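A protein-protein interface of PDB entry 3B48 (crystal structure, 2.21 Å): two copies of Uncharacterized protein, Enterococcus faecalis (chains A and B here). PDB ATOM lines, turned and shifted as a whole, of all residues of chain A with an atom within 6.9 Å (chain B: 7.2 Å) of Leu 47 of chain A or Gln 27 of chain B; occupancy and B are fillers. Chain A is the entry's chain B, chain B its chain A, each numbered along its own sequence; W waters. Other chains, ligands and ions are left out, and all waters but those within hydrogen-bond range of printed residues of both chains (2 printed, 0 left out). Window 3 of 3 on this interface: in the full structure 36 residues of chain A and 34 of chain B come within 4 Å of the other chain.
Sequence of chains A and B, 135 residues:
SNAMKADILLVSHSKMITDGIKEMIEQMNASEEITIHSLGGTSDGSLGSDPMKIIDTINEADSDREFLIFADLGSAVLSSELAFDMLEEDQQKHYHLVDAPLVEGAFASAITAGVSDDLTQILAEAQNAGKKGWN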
ATOM      1  N   SER A  12      18.235  19.634 -25.955  1.00  0.00           N
ATOM      2  CA  SER A  12      18.343  18.631 -24.912  1.00  0.00           C
ATOM      3  C   SER A  12      19.744  18.700 -24.381  1.00  0.00           C
ATOM      4  O   SER A  12      20.583  19.270 -25.038  1.00  0.00           O
ATOM      5  CB  SER A  12      18.058  17.233 -25.506  1.00  0.00           C
ATOM      6  OG  SER A  12      18.107  16.210 -24.525  1.00  0.00           O
ATOM      7  N   HIS A  13      20.007  18.112 -23.212  1.00  0.00           N
ATOM      8  CA  HIS A  13      21.391  17.733 -22.865  1.00  0.00           C
ATOM      9  C   HIS A  13      22.001  16.710 -23.826  1.00  0.00           C
ATOM     10  O   HIS A  13      23.169  16.737 -24.078  1.00  0.00           O
ATOM     11  CB  HIS A  13      21.474  17.169 -21.450  1.00  0.00           C
ATOM     12  CG  HIS A  13      21.553  18.214 -20.392  1.00  0.00           C
ATOM     13  ND1 HIS A  13      22.290  18.048 -19.239  1.00  0.00           N
ATOM     14  CD2 HIS A  13      21.005  19.448 -20.316  1.00  0.00           C
ATOM     15  CE1 HIS A  13      22.185  19.134 -18.496  1.00  0.00           C
ATOM     16  NE2 HIS A  13      21.408  19.997 -19.129  1.00  0.00           N
ATOM     17  N   SER A  14      21.182  15.809 -24.351  1.00  0.00           N
ATOM     18  CA  SER A  14      21.656  14.646 -25.106  1.00  0.00           C
ATOM     19  C   SER A  14      21.511  14.914 -26.586  1.00  0.00           C
ATOM     20  O   SER A  14      20.406  15.179 -27.066  1.00  0.00           O
ATOM     21  CB  SER A  14      20.846  13.394 -24.689  1.00  0.00           C
ATOM     22  OG  SER A  14      21.038  12.256 -25.518  1.00  0.00           O
ATOM     23  N   LYS A  15      22.646  14.865 -27.289  1.00  0.00           N
ATOM     24  CA  LYS A  15      22.685  14.900 -28.746  1.00  0.00           C
ATOM     25  C   LYS A  15      22.121  13.585 -29.282  1.00  0.00           C
ATOM     26  O   LYS A  15      21.494  13.559 -30.343  1.00  0.00           O
ATOM     27  CB  LYS A  15      24.106  15.166 -29.276  1.00  0.00           C
ATOM     28  CG  LYS A  15      24.184  15.196 -30.832  1.00  0.00           C
ATOM     29  CD  LYS A  15      25.549  15.716 -31.361  1.00  0.00           C
ATOM     30  CE  LYS A  15      25.860  15.282 -32.813  1.00  0.00           C
ATOM     31  NZ  LYS A  15      25.058  16.016 -33.860  1.00  0.00           N
ATOM     32  N   MET A  16      22.319  12.500 -28.546  1.00  0.00           N
ATOM     33  CA  MET A  16      21.685  11.237 -28.928  1.00  0.00           C
ATOM     34  C   MET A  16      20.157  11.336 -29.054  1.00  0.00           C
ATOM     35  O   MET A  16      19.565  10.826 -30.029  1.00  0.00           O
ATOM     36  CB  MET A  16      22.030  10.130 -27.950  1.00  0.00           C
ATOM     37  CG  MET A  16      23.151   9.263 -28.363  1.00  0.00           C
ATOM     38  SD  MET A  16      22.996   7.620 -27.307  1.00  0.00           S
ATOM     39  CE  MET A  16      22.592   6.367 -28.786  1.00  0.00           C
ATOM     40  N   GLY A  41      23.135  18.714 -26.826  1.00  0.00           N
ATOM     41  CA  GLY A  41      24.532  18.639 -26.491  1.00  0.00           C
ATOM     42  C   GLY A  41      25.202  19.992 -26.441  1.00  0.00           C
ATOM     43  O   GLY A  41      24.637  21.009 -26.855  1.00  0.00           O
ATOM     44  N   THR A  42      26.405  20.017 -25.899  1.00  0.00           N
ATOM     45  CA  THR A  42      27.210  21.207 -25.972  1.00  0.00           C
ATOM     46  C   THR A  42      27.899  21.263 -27.337  1.00  0.00           C
ATOM     47  O   THR A  42      27.769  20.343 -28.146  1.00  0.00           O
ATOM     48  CB  THR A  42      28.265  21.235 -24.857  1.00  0.00           C
ATOM     49  OG1 THR A  42      29.285  20.270 -25.149  1.00  0.00           O
ATOM     50  CG2 THR A  42      27.601  20.945 -23.493  1.00  0.00           C
ATOM     51  N   ASP A  44      30.465  20.414 -28.444  1.00  0.00           N
ATOM     52  CA  ASP A  44      31.345  19.285 -28.779  1.00  0.00           C
ATOM     53  C   ASP A  44      30.712  17.906 -28.564  1.00  0.00           C
ATOM     54  O   ASP A  44      31.422  16.887 -28.516  1.00  0.00           O
ATOM     55  CB  ASP A  44      32.687  19.400 -28.032  1.00  0.00           C
ATOM     56  CG  ASP A  44      32.565  19.163 -26.521  1.00  0.00           C
ATOM     57  OD1 ASP A  44      31.443  19.180 -25.961  1.00  0.00           O
ATOM     58  OD2 ASP A  44      33.619  18.949 -25.889  1.00  0.00           O
ATOM     59  N   GLY A  45      29.389  17.885 -28.416  1.00  0.00           N
ATOM     60  CA  GLY A  45      28.651  16.637 -28.197  1.00  0.00           C
ATOM     61  C   GLY A  45      28.404  16.229 -26.757  1.00  0.00           C
ATOM     62  O   GLY A  45      27.616  15.325 -26.507  1.00  0.00           O
ATOM     63  N   SER A  46      29.086  16.877 -25.812  1.00  0.00           N
ATOM     64  CA  SER A  46      28.916  16.606 -24.378  1.00  0.00           C
ATOM     65  C   SER A  46      27.482  16.769 -23.897  1.00  0.00           C
ATOM     66  O   SER A  46      26.713  17.501 -24.517  1.00  0.00           O
ATOM     67  CB  SER A  46      29.808  17.517 -23.547  1.00  0.00           C
ATOM     68  OG  SER A  46      31.112  16.989 -23.470  1.00  0.00           O
ATOM     69  N   LEU A  47      27.137  16.092 -22.793  1.00  0.00           N
ATOM     70  CA  LEU A  47      25.816  16.259 -22.172  1.00  0.00           C
ATOM     71  C   LEU A  47      25.715  17.679 -21.601  1.00  0.00           C
ATOM     72  O   LEU A  47      26.509  18.055 -20.736  1.00  0.00           O
ATOM     73  CB  LEU A  47      25.552  15.204 -21.073  1.00  0.00           C
ATOM     74  CG  LEU A  47      25.266  13.756 -21.536  1.00  0.00           C
ATOM     75  CD1 LEU A  47      25.643  12.704 -20.463  1.00  0.00           C
ATOM     76  CD2 LEU A  47      23.838  13.570 -21.997  1.00  0.00           C
ATOM     77  N   GLY A  48      24.761  18.459 -22.107  1.00  0.00           N
ATOM     78  CA  GLY A  48      24.586  19.844 -21.690  1.00  0.00           C
ATOM     79  C   GLY A  48      23.926  20.651 -22.788  1.00  0.00           C
ATOM     80  O   GLY A  48      23.682  20.143 -23.879  1.00  0.00           O
ATOM     81  N   SER A  49      23.607  21.909 -22.523  1.00  0.00           N
ATOM     82  CA  SER A  49      22.980  22.705 -23.575  1.00  0.00           C
ATOM     83  C   SER A  49      23.661  24.044 -23.824  1.00  0.00           C
ATOM     84  O   SER A  49      24.166  24.654 -22.903  1.00  0.00           O
ATOM     85  CB  SER A  49      21.489  22.879 -23.288  1.00  0.00           C
ATOM     86  OG  SER A  49      20.856  21.632 -23.534  1.00  0.00           O
ATOM     87  N   SER A  75      18.710  22.571 -18.269  1.00  0.00           N
ATOM     88  CA  SER A  75      19.406  23.697 -18.844  1.00  0.00           C
ATOM     89  C   SER A  75      19.036  23.834 -20.311  1.00  0.00           C
ATOM     90  O   SER A  75      19.238  24.886 -20.906  1.00  0.00           O
ATOM     91  CB  SER A  75      20.927  23.540 -18.667  1.00  0.00           C
ATOM     92  OG  SER A  75      21.445  22.571 -19.567  1.00  0.00           O
ATOM     93  N   ASP B  19      18.446   4.831 -25.648  1.00  0.00           N
ATOM     94  CA  ASP B  19      19.858   4.878 -25.211  1.00  0.00           C
ATOM     95  C   ASP B  19      20.225   6.259 -24.666  1.00  0.00           C
ATOM     96  O   ASP B  19      20.782   6.343 -23.576  1.00  0.00           O
ATOM     97  CB  ASP B  19      20.834   4.533 -26.357  1.00  0.00           C
ATOM     98  CG  ASP B  19      20.897   3.035 -26.670  1.00  0.00           C
ATOM     99  OD1 ASP B  19      20.153   2.238 -26.022  1.00  0.00           O
ATOM    100  OD2 ASP B  19      21.703   2.647 -27.557  1.00  0.00           O
ATOM    101  N   GLY B  20      19.889   7.310 -25.435  1.00  0.00           N
ATOM    102  CA  GLY B  20      20.064   8.695 -25.046  1.00  0.00           C
ATOM    103  C   GLY B  20      19.418   9.102 -23.725  1.00  0.00           C
ATOM    104  O   GLY B  20      20.053   9.783 -22.903  1.00  0.00           O
ATOM    105  N   ILE B  21      18.160   8.697 -23.524  1.00  0.00           N
ATOM    106  CA  ILE B  21      17.429   8.949 -22.266  1.00  0.00           C
ATOM    107  C   ILE B  21      18.062   8.201 -21.075  1.00  0.00           C
ATOM    108  O   ILE B  21      18.266   8.784 -20.014  1.00  0.00           O
ATOM    109  CB  ILE B  21      15.969   8.502 -22.348  1.00  0.00           C
ATOM    110  CG1 ILE B  21      15.159   9.377 -23.305  1.00  0.00           C
ATOM    111  CG2 ILE B  21      15.304   8.472 -20.932  1.00  0.00           C
ATOM    112  CD1 ILE B  21      13.894   8.648 -23.758  1.00  0.00           C
ATOM    113  N   LYS B  22      18.371   6.915 -21.277  1.00  0.00           N
ATOM    114  CA  LYS B  22      19.055   6.103 -20.282  1.00  0.00           C
ATOM    115  C   LYS B  22      20.388   6.713 -19.847  1.00  0.00           C
ATOM    116  O   LYS B  22      20.668   6.856 -18.651  1.00  0.00           O
ATOM    117  CB  LYS B  22      19.260   4.692 -20.810  1.00  0.00           C
ATOM    118  CG  LYS B  22      20.210   3.858 -19.979  1.00  0.00           C
ATOM    119  CD  LYS B  22      20.123   2.388 -20.379  1.00  0.00           C
ATOM    120  CE  LYS B  22      21.268   1.601 -19.784  1.00  0.00           C
ATOM    121  NZ  LYS B  22      20.944   1.301 -18.372  1.00  0.00           N
ATOM    122  N   GLU B  23      21.200   7.091 -20.818  1.00  0.00           N
ATOM    123  CA  GLU B  23      22.496   7.667 -20.538  1.00  0.00           C
ATOM    124  C   GLU B  23      22.350   9.027 -19.829  1.00  0.00           C
ATOM    125  O   GLU B  23      23.137   9.372 -18.948  1.00  0.00           O
ATOM    126  CB  GLU B  23      23.306   7.774 -21.831  1.00  0.00           C
ATOM    127  CG  GLU B  23      24.119   9.035 -21.922  1.00  0.00           C
ATOM    128  CD  GLU B  23      25.100   9.031 -23.075  1.00  0.00           C
ATOM    129  OE1 GLU B  23      24.682   9.377 -24.214  1.00  0.00           O
ATOM    130  OE2 GLU B  23      26.293   8.696 -22.826  1.00  0.00           O
ATOM    131  N   MET B  24      21.326   9.789 -20.187  1.00  0.00           N
ATOM    132  CA  MET B  24      21.142  11.084 -19.573  1.00  0.00           C
ATOM    133  C   MET B  24      20.680  10.966 -18.121  1.00  0.00           C
ATOM    134  O   MET B  24      21.175  11.681 -17.266  1.00  0.00           O
ATOM    135  CB  MET B  24      20.163  11.908 -20.383  1.00  0.00           C
ATOM    136  CG  MET B  24      20.407  13.409 -20.343  1.00  0.00           C
ATOM    137  SD  MET B  24      18.884  14.294 -21.220  1.00  0.00           S
ATOM    138  CE  MET B  24      17.377  13.383 -20.320  1.00  0.00           C
ATOM    139  N   ILE B  25      19.744  10.064 -17.841  1.00  0.00           N
ATOM    140  CA  ILE B  25      19.306   9.810 -16.461  1.00  0.00           C
ATOM    141  C   ILE B  25      20.470   9.397 -15.548  1.00  0.00           C
ATOM    142  O   ILE B  25      20.648   9.932 -14.451  1.00  0.00           O
ATOM    143  CB  ILE B  25      18.194   8.724 -16.414  1.00  0.00           C
ATOM    144  CG1 ILE B  25      16.895   9.270 -17.018  1.00  0.00           C
ATOM    145  CG2 ILE B  25      17.962   8.207 -14.970  1.00  0.00           C
ATOM    146  CD1 ILE B  25      15.822   8.226 -17.214  1.00  0.00           C
ATOM    147  N   GLU B  26      21.262   8.445 -16.023  1.00  0.00           N
ATOM    148  CA  GLU B  26      22.345   7.867 -15.239  1.00  0.00           C
ATOM    149  C   GLU B  26      23.452   8.866 -14.905  1.00  0.00           C
ATOM    150  O   GLU B  26      24.003   8.849 -13.801  1.00  0.00           O
ATOM    151  CB  GLU B  26      22.925   6.661 -15.974  1.00  0.00           C
ATOM    152  CG  GLU B  26      21.965   5.511 -16.087  1.00  0.00           C
ATOM    153  CD  GLU B  26      22.479   4.399 -16.986  1.00  0.00           C
ATOM    154  OE1 GLU B  26      23.483   4.610 -17.718  1.00  0.00           O
ATOM    155  OE2 GLU B  26      21.862   3.305 -16.957  1.00  0.00           O
ATOM    156  N   GLN B  27      23.751   9.736 -15.863  1.00  0.00           N
ATOM    157  CA  GLN B  27      24.870  10.679 -15.746  1.00  0.00           C
ATOM    158  C   GLN B  27      24.589  11.833 -14.786  1.00  0.00           C
ATOM    159  O   GLN B  27      25.472  12.635 -14.501  1.00  0.00           O
ATOM    160  CB  GLN B  27      25.285  11.200 -17.127  1.00  0.00           C
ATOM    161  CG  GLN B  27      26.391  10.377 -17.800  1.00  0.00           C
ATOM    162  CD  GLN B  27      25.901   9.045 -18.402  1.00  0.00           C
ATOM    163  OE1 GLN B  27      25.253   8.232 -17.727  1.00  0.00           O
ATOM    164  NE2 GLN B  27      26.238   8.812 -19.678  1.00  0.00           N
ATOM    165  N   MET B  28      23.370  11.882 -14.265  1.00  0.00           N
ATOM    166  CA  MET B  28      22.915  13.004 -13.455  1.00  0.00           C
ATOM    167  C   MET B  28      22.434  12.587 -12.070  1.00  0.00           C
ATOM    168  O   MET B  28      22.345  13.412 -11.161  1.00  0.00           O
ATOM    169  CB  MET B  28      21.774  13.723 -14.176  1.00  0.00           C
ATOM    170  CG  MET B  28      22.121  14.248 -15.569  1.00  0.00           C
ATOM    171  SD  MET B  28      20.545  14.973 -16.489  1.00  0.00           S
ATOM    172  CE  MET B  28      20.174  16.489 -15.279  1.00  0.00           C
ATOM    173  N   ASN B  29      22.116  11.308 -11.917  1.00  0.00           N
ATOM    174  CA  ASN B  29      21.373  10.840 -10.754  1.00  0.00           C
ATOM    175  C   ASN B  29      22.095   9.744  -9.986  1.00  0.00           C
ATOM    176  O   ASN B  29      22.116   8.590 -10.407  1.00  0.00           O
ATOM    177  CB  ASN B  29      19.967  10.381 -11.181  1.00  0.00           C
ATOM    178  CG  ASN B  29      19.133  11.510 -11.803  1.00  0.00           C
ATOM    179  OD1 ASN B  29      19.579  12.659 -11.893  1.00  0.00           O
ATOM    180  ND2 ASN B  29      17.910  11.179 -12.232  1.00  0.00           N
HETATM  181  O   HOH W   1      22.513  11.017 -23.948  1.00  0.00           O
HETATM  182  O   HOH W   2      18.108  17.850 -21.209  1.00  0.00           O
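N of Gly 20 of chain B lies within hydrogen-bond range of SD of Met 16 of chain A (3.6 Å).
The backbone NH (N) of Ser 14 of chain A lies within hydrogen-bond range of the side-chain hydroxyl (OG) of Ser 12 of chain A (3.1 Å). The backbone carbonyl oxygen (O) of His 13 of chain A sits at hydrogen-bond distance from the backbone NH (N) of Gly 48 of chain A. NE2 of His 13 of chain A lies within hydrogen-bond range of OG of Ser 75 of chain A (2.6 Å). The backbone carbonyl oxygen (O) of His 13 of chain A sits close to the backbone NH (N) of Gly 41 of chain A (3.4 Å). The side-chain hydroxyl (OG) of Ser 49 of chain A lies within hydrogen-bond range of the backbone carbonyl oxygen (O) of Ser 12 of chain A, 2.8 Å away. The backbone carbonyl oxygen (O) of Glu 23 of chain B sits close to the side-chain amide oxygen (OE1) of Gln 27 of chain B (2.7 Å).
Among the printed residues, pairs that only touch across the chains: Ser 12 of chain A with Met 24 of chain B (3.9 Å), His 13 of chain A with Met 24 of chain B (3.9 Å), Ser 14 of chain A with Gly 20 of chain B (3.7 Å), Met 16 of chain A with Asp 19 of chain B (3.5 Å), Met 16 of chain A with Glu 23 of chain B (3.9 Å), Leu 47 of chain A with Met 24 of chain B (3.8 Å) and Leu 47 of chain A with Gln 27 of chain B (3.6 Å).
Of the printed residues of chain B, Ser 12 of chain A touches Met 24 (3.9 Å). Gly 45 of chain A touches none of the printed residues of chain B. Printed residues of chain B within 4 Å of Leu 47 of chain A: Met 24 (3.8 Å) and Gln 27 (3.6 Å). Gly 48 of chain A touches none of the printed residues of chain B. Of the printed residues of chain A, Gly 20 of chain B touches Ser 14 and Met 16. Of the printed residues of chain A, Glu 23 of chain B touches Met 16. Gln 27 of chain B touches just one residue of chain A: Leu 47. The nearest printed residue of chain A that does not touch Gln 27 of chain B is His 13 of chain A (7.8 Å). The nearest printed residue of chain B that does not touch Met 16 of chain A is Ile 21 of chain B (6.1 Å).
Of the 11 printed residues of chain B, 5 touch a printed residue of chain A. Hydrophobic or aromatic side chains of chain B within 4 Å of the printed part of chain A: Met 24. Hydrophobic or aromatic side chains of chain A within 4 Å of the printed part of chain B: His 13, Met 16 and Leu 47. Along chain A the printed residues that touch a printed residue of chain B span positions 12 to 47. Among the printed residues, 8 pairs touch across the chains. Among the printed residues, no Asp or Glu carboxylate lies within 4 Å of a Lys or Arg side-chain nitrogen of the other chain.
No position is printed for both chains. Of the 8 pairs that touch across the chains among the printed residues, none has its exchanged pair printed and touching as well.
Water W1 lies within hydrogen-bond range of OG of Ser 14 of chain A (2.5 Å), OE1 of Glu 23 of chain B (2.7 Å) and O of Gly 20 of chain B (2.9 Å). Water W2 lies within hydrogen-bond range of the backbone NH (N) of His 13 of chain A (2.8 Å) and the side-chain sulfur (SD) of Met 24 of chain B (3.6 Å).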
